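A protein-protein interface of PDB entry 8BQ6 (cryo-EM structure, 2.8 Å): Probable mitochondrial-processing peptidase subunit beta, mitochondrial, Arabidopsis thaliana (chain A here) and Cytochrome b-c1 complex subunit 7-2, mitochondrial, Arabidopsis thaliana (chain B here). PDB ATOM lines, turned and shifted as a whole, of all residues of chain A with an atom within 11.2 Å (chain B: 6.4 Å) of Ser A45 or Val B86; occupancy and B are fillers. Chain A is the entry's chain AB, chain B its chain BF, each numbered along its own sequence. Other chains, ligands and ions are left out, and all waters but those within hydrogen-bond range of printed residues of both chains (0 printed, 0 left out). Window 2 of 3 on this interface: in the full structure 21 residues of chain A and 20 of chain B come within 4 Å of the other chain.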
ATOM      1  N   SER A  45     -15.800   3.388 -30.545  1.00  0.00           N
ATOM      2  CA  SER A  45     -14.733   2.440 -30.248  1.00  0.00           C
ATOM      3  C   SER A  45     -15.104   1.553 -29.063  1.00  0.00           C
ATOM      4  O   SER A  45     -15.753   2.011 -28.124  1.00  0.00           O
ATOM      5  CB  SER A  45     -13.423   3.178 -29.968  1.00  0.00           C
ATOM      6  OG  SER A  45     -13.423   3.750 -28.672  1.00  0.00           O
ATOM      7  N   PRO A  46     -14.706   0.285 -29.115  1.00  0.00           N
ATOM      8  CA  PRO A  46     -14.952  -0.622 -27.987  1.00  0.00           C
ATOM      9  C   PRO A  46     -14.102  -0.246 -26.788  1.00  0.00           C
ATOM     10  O   PRO A  46     -13.001   0.305 -26.942  1.00  0.00           O
ATOM     11  CB  PRO A  46     -14.558  -2.003 -28.536  1.00  0.00           C
ATOM     12  CG  PRO A  46     -14.156  -1.802 -29.960  1.00  0.00           C
ATOM     13  CD  PRO A  46     -13.940  -0.353 -30.195  1.00  0.00           C
ATOM     14  N   PRO A  47     -14.578  -0.528 -25.575  1.00  0.00           N
ATOM     15  CA  PRO A  47     -13.796  -0.189 -24.390  1.00  0.00           C
ATOM     16  C   PRO A  47     -12.541  -1.035 -24.307  1.00  0.00           C
ATOM     17  O   PRO A  47     -12.504  -2.172 -24.808  1.00  0.00           O
ATOM     18  CB  PRO A  47     -14.759  -0.499 -23.230  1.00  0.00           C
ATOM     19  CG  PRO A  47     -15.724  -1.481 -23.790  1.00  0.00           C
ATOM     20  CD  PRO A  47     -15.881  -1.126 -25.235  1.00  0.00           C
ATOM     21  N   PRO A  48     -11.484  -0.525 -23.681  1.00  0.00           N
ATOM     22  CA  PRO A  48     -10.309  -1.356 -23.404  1.00  0.00           C
ATOM     23  C   PRO A  48     -10.661  -2.450 -22.413  1.00  0.00           C
ATOM     24  O   PRO A  48     -11.619  -2.306 -21.638  1.00  0.00           O
ATOM     25  CB  PRO A  48      -9.307  -0.360 -22.806  1.00  0.00           C
ATOM     26  CG  PRO A  48     -10.150   0.706 -22.213  1.00  0.00           C
ATOM     27  CD  PRO A  48     -11.389   0.805 -23.057  1.00  0.00           C
ATOM     28  N   PRO A  49      -9.916  -3.559 -22.399  1.00  0.00           N
ATOM     29  CA  PRO A  49     -10.329  -4.700 -21.573  1.00  0.00           C
ATOM     30  C   PRO A  49      -9.980  -4.556 -20.102  1.00  0.00           C
ATOM     31  O   PRO A  49      -9.538  -5.521 -19.472  1.00  0.00           O
ATOM     32  CB  PRO A  49      -9.557  -5.865 -22.196  1.00  0.00           C
ATOM     33  CG  PRO A  49      -8.300  -5.229 -22.682  1.00  0.00           C
ATOM     34  CD  PRO A  49      -8.656  -3.826 -23.114  1.00  0.00           C
ATOM     35  N   LEU A  51     -12.030  -1.696 -18.470  1.00  0.00           N
ATOM     36  CA  LEU A  51     -12.934  -0.615 -18.101  1.00  0.00           C
ATOM     37  C   LEU A  51     -14.200  -1.148 -17.446  1.00  0.00           C
ATOM     38  O   LEU A  51     -14.544  -0.761 -16.324  1.00  0.00           O
ATOM     39  CB  LEU A  51     -13.281   0.211 -19.340  1.00  0.00           C
ATOM     40  CG  LEU A  51     -13.898   1.580 -19.075  1.00  0.00           C
ATOM     41  CD1 LEU A  51     -13.152   2.309 -17.959  1.00  0.00           C
ATOM     42  CD2 LEU A  51     -13.918   2.394 -20.353  1.00  0.00           C
ATOM     43  N   MET A  52     -14.919  -2.017 -18.144  1.00  0.00           N
ATOM     44  CA  MET A  52     -16.107  -2.612 -17.562  1.00  0.00           C
ATOM     45  C   MET A  52     -15.705  -3.542 -16.420  1.00  0.00           C
ATOM     46  O   MET A  52     -14.682  -4.228 -16.509  1.00  0.00           O
ATOM     47  CB  MET A  52     -16.902  -3.379 -18.616  1.00  0.00           C
ATOM     48  CG  MET A  52     -17.267  -2.552 -19.838  1.00  0.00           C
ATOM     49  SD  MET A  52     -17.970  -0.942 -19.430  1.00  0.00           S
ATOM     50  CE  MET A  52     -19.421  -1.431 -18.503  1.00  0.00           C
ATOM     51  N   TYR A  54     -16.812  -6.397 -15.455  1.00  0.00           N
ATOM     52  CA  TYR A  54     -16.763  -7.819 -15.774  1.00  0.00           C
ATOM     53  C   TYR A  54     -15.579  -8.148 -16.675  1.00  0.00           C
ATOM     54  O   TYR A  54     -15.043  -9.260 -16.617  1.00  0.00           O
ATOM     55  CB  TYR A  54     -18.077  -8.270 -16.411  1.00  0.00           C
ATOM     56  CG  TYR A  54     -18.589  -7.369 -17.505  1.00  0.00           C
ATOM     57  CD1 TYR A  54     -18.218  -7.570 -18.824  1.00  0.00           C
ATOM     58  CD2 TYR A  54     -19.451  -6.322 -17.219  1.00  0.00           C
ATOM     59  CE1 TYR A  54     -18.685  -6.754 -19.826  1.00  0.00           C
ATOM     60  CE2 TYR A  54     -19.923  -5.501 -18.215  1.00  0.00           C
ATOM     61  CZ  TYR A  54     -19.537  -5.721 -19.517  1.00  0.00           C
ATOM     62  OH  TYR A  54     -20.006  -4.901 -20.514  1.00  0.00           O
ATOM     63  N   ASP A  55     -15.152  -7.202 -17.515  1.00  0.00           N
ATOM     64  CA  ASP A  55     -13.969  -7.445 -18.334  1.00  0.00           C
ATOM     65  C   ASP A  55     -12.708  -7.456 -17.486  1.00  0.00           C
ATOM     66  O   ASP A  55     -11.809  -8.276 -17.705  1.00  0.00           O
ATOM     67  CB  ASP A  55     -13.847  -6.402 -19.439  1.00  0.00           C
ATOM     68  CG  ASP A  55     -14.729  -6.709 -20.619  1.00  0.00           C
ATOM     69  OD1 ASP A  55     -15.263  -7.834 -20.681  1.00  0.00           O
ATOM     70  OD2 ASP A  55     -14.863  -5.840 -21.502  1.00  0.00           O
ATOM     71  N   ARG B  29     -21.583  -9.565 -33.817  1.00  0.00           N
ATOM     72  CA  ARG B  29     -21.705  -8.171 -33.406  1.00  0.00           C
ATOM     73  C   ARG B  29     -23.139  -7.668 -33.524  1.00  0.00           C
ATOM     74  O   ARG B  29     -23.563  -6.813 -32.739  1.00  0.00           O
ATOM     75  CB  ARG B  29     -20.756  -7.314 -34.241  1.00  0.00           C
ATOM     76  CG  ARG B  29     -20.839  -5.836 -33.972  1.00  0.00           C
ATOM     77  CD  ARG B  29     -19.882  -5.074 -34.864  1.00  0.00           C
ATOM     78  NE  ARG B  29     -18.545  -5.649 -34.820  1.00  0.00           N
ATOM     79  CZ  ARG B  29     -17.588  -5.247 -33.996  1.00  0.00           C
ATOM     80  NH1 ARG B  29     -17.789  -4.266 -33.131  1.00  0.00           N
ATOM     81  NH2 ARG B  29     -16.401  -5.843 -34.039  1.00  0.00           N
ATOM     82  N   ASP B  81     -26.588   0.712 -34.427  1.00  0.00           N
ATOM     83  CA  ASP B  81     -25.222   0.848 -34.923  1.00  0.00           C
ATOM     84  C   ASP B  81     -24.290   1.408 -33.860  1.00  0.00           C
ATOM     85  O   ASP B  81     -23.112   1.038 -33.803  1.00  0.00           O
ATOM     86  CB  ASP B  81     -25.202   1.727 -36.169  1.00  0.00           C
ATOM     87  CG  ASP B  81     -26.215   1.292 -37.194  1.00  0.00           C
ATOM     88  OD1 ASP B  81     -26.201   0.096 -37.558  1.00  0.00           O
ATOM     89  OD2 ASP B  81     -27.020   2.136 -37.636  1.00  0.00           O
ATOM     90  N   ASN B  82     -24.790   2.309 -33.014  1.00  0.00           N
ATOM     91  CA  ASN B  82     -23.951   2.851 -31.953  1.00  0.00           C
ATOM     92  C   ASN B  82     -23.528   1.763 -30.979  1.00  0.00           C
ATOM     93  O   ASN B  82     -22.371   1.718 -30.548  1.00  0.00           O
ATOM     94  CB  ASN B  82     -24.682   3.974 -31.224  1.00  0.00           C
ATOM     95  CG  ASN B  82     -24.306   5.337 -31.749  1.00  0.00           C
ATOM     96  OD1 ASN B  82     -24.038   5.501 -32.939  1.00  0.00           O
ATOM     97  ND2 ASN B  82     -24.275   6.324 -30.864  1.00  0.00           N
ATOM     98  N   LEU B  83     -24.452   0.870 -30.626  1.00  0.00           N
ATOM     99  CA  LEU B  83     -24.109  -0.219 -29.722  1.00  0.00           C
ATOM    100  C   LEU B  83     -23.203  -1.234 -30.409  1.00  0.00           C
ATOM    101  O   LEU B  83     -22.280  -1.770 -29.787  1.00  0.00           O
ATOM    102  CB  LEU B  83     -25.384  -0.881 -29.204  1.00  0.00           C
ATOM    103  CG  LEU B  83     -26.005  -0.223 -27.968  1.00  0.00           C
ATOM    104  CD1 LEU B  83     -27.340  -0.867 -27.649  1.00  0.00           C
ATOM    105  CD2 LEU B  83     -25.074  -0.293 -26.770  1.00  0.00           C
ATOM    106  N   GLN B  84     -23.437  -1.493 -31.698  1.00  0.00           N
ATOM    107  CA  GLN B  84     -22.588  -2.426 -32.431  1.00  0.00           C
ATOM    108  C   GLN B  84     -21.143  -1.948 -32.484  1.00  0.00           C
ATOM    109  O   GLN B  84     -20.219  -2.768 -32.488  1.00  0.00           O
ATOM    110  CB  GLN B  84     -23.131  -2.631 -33.844  1.00  0.00           C
ATOM    111  CG  GLN B  84     -24.408  -3.443 -33.892  1.00  0.00           C
ATOM    112  CD  GLN B  84     -24.757  -3.920 -35.286  1.00  0.00           C
ATOM    113  OE1 GLN B  84     -23.936  -4.523 -35.976  1.00  0.00           O
ATOM    114  NE2 GLN B  84     -25.985  -3.652 -35.708  1.00  0.00           N
ATOM    115  N   ALA B  85     -20.926  -0.632 -32.520  1.00  0.00           N
ATOM    116  CA  ALA B  85     -19.574  -0.098 -32.626  1.00  0.00           C
ATOM    117  C   ALA B  85     -18.717  -0.398 -31.403  1.00  0.00           C
ATOM    118  O   ALA B  85     -17.489  -0.425 -31.521  1.00  0.00           O
ATOM    119  CB  ALA B  85     -19.626   1.411 -32.865  1.00  0.00           C
ATOM    120  N   VAL B  86     -19.324  -0.627 -30.237  1.00  0.00           N
ATOM    121  CA  VAL B  86     -18.572  -0.848 -29.007  1.00  0.00           C
ATOM    122  C   VAL B  86     -18.504  -2.324 -28.628  1.00  0.00           C
ATOM    123  O   VAL B  86     -18.011  -2.658 -27.547  1.00  0.00           O
ATOM    124  CB  VAL B  86     -19.144  -0.014 -27.851  1.00  0.00           C
ATOM    125  CG1 VAL B  86     -19.293   1.430 -28.279  1.00  0.00           C
ATOM    126  CG2 VAL B  86     -20.479  -0.575 -27.399  1.00  0.00           C
ATOM    127  N   GLN B  87     -18.977  -3.216 -29.492  1.00  0.00           N
ATOM    128  CA  GLN B  87     -18.959  -4.641 -29.194  1.00  0.00           C
ATOM    129  C   GLN B  87     -17.568  -5.224 -29.412  1.00  0.00           C
ATOM    130  O   GLN B  87     -16.822  -4.776 -30.288  1.00  0.00           O
ATOM    131  CB  GLN B  87     -19.975  -5.375 -30.066  1.00  0.00           C
ATOM    132  CG  GLN B  87     -21.420  -4.965 -29.838  1.00  0.00           C
ATOM    133  CD  GLN B  87     -21.811  -4.983 -28.376  1.00  0.00           C
ATOM    134  OE1 GLN B  87     -21.710  -6.011 -27.711  1.00  0.00           O
ATOM    135  NE2 GLN B  87     -22.287  -3.851 -27.875  1.00  0.00           N
ATOM    136  N   THR B  88     -17.219  -6.237 -28.608  1.00  0.00           N
ATOM    137  CA  THR B  88     -15.941  -6.946 -28.705  1.00  0.00           C
ATOM    138  C   THR B  88     -16.225  -8.437 -28.850  1.00  0.00           C
ATOM    139  O   THR B  88     -16.094  -9.201 -27.883  1.00  0.00           O
ATOM    140  CB  THR B  88     -15.049  -6.697 -27.490  1.00  0.00           C
ATOM    141  OG1 THR B  88     -15.559  -7.423 -26.366  1.00  0.00           O
ATOM    142  CG2 THR B  88     -14.995  -5.228 -27.147  1.00  0.00           C
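The guanidinium group (NH1) of Arg B29 is in hydrogen-bond range of the backbone carbonyl oxygen (O) of Gln B87, 3.0 Å away. The backbone carbonyl oxygen of Leu B83 sits at hydrogen-bond distance from the side-chain amide nitrogen of Gln B87 (2.8 Å).
Among the printed residues, pairs that only touch across the chains: Ser A45 with Ala B85 (3.96 Å), Ser A45 with Val B86 (3.6 Å), Pro A46 with Ala B85 (3.7 Å), Pro A46 with Val B86 (3.7 Å), Pro A46 with Gln B87 (3.99 Å), Pro A46 with Thr B88 (3.5 Å) and Pro A47 with Val B86 (3.5 Å).
Of chain B, only Ala B85 and Val B86 come within 4 Å of Ser A45. Of the printed residues of chain B, Pro A46 touches Ala B85 (3.7 Å), Val B86 (3.7 Å), Gln B87 (3.99 Å) and Thr B88 (3.5 Å). Printed residues of chain B within 4 Å of Pro A47: Val B86. Asp A55 touches none of the printed residues of chain B. Of chain A, only Ser A45 (3.6 Å), Pro A46 (3.7 Å) and Pro A47 (3.5 Å) come within 4 Å of Val B86. Of the printed residues of chain A, Gln B87 touches Pro A46. Of chain A, only Pro A46 comes within 4 Å of Thr B88. The nearest residue of chain B that does not touch Ser A45 is Gln B87 (6.2 Å).
Of the 9 printed residues of chain A, 3 touch a printed residue of chain B. Printed residues of chain A that touch a printed residue of chain B: Ser A45, Pro A46 and Pro A47. Hydrophobic or aromatic side chains of chain A that line the printed part of chain B: Pro A46 and Pro A47. Of the 9 printed residues of chain B, 4 touch a printed residue of chain A. Hydrophobic or aromatic side chains of chain B within 4 Å of the printed part of chain A: Val B86. Among the printed residues, no Asp or Glu carboxylate lies within 4 Å of a Lys or Arg side-chain nitrogen of the other chain.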
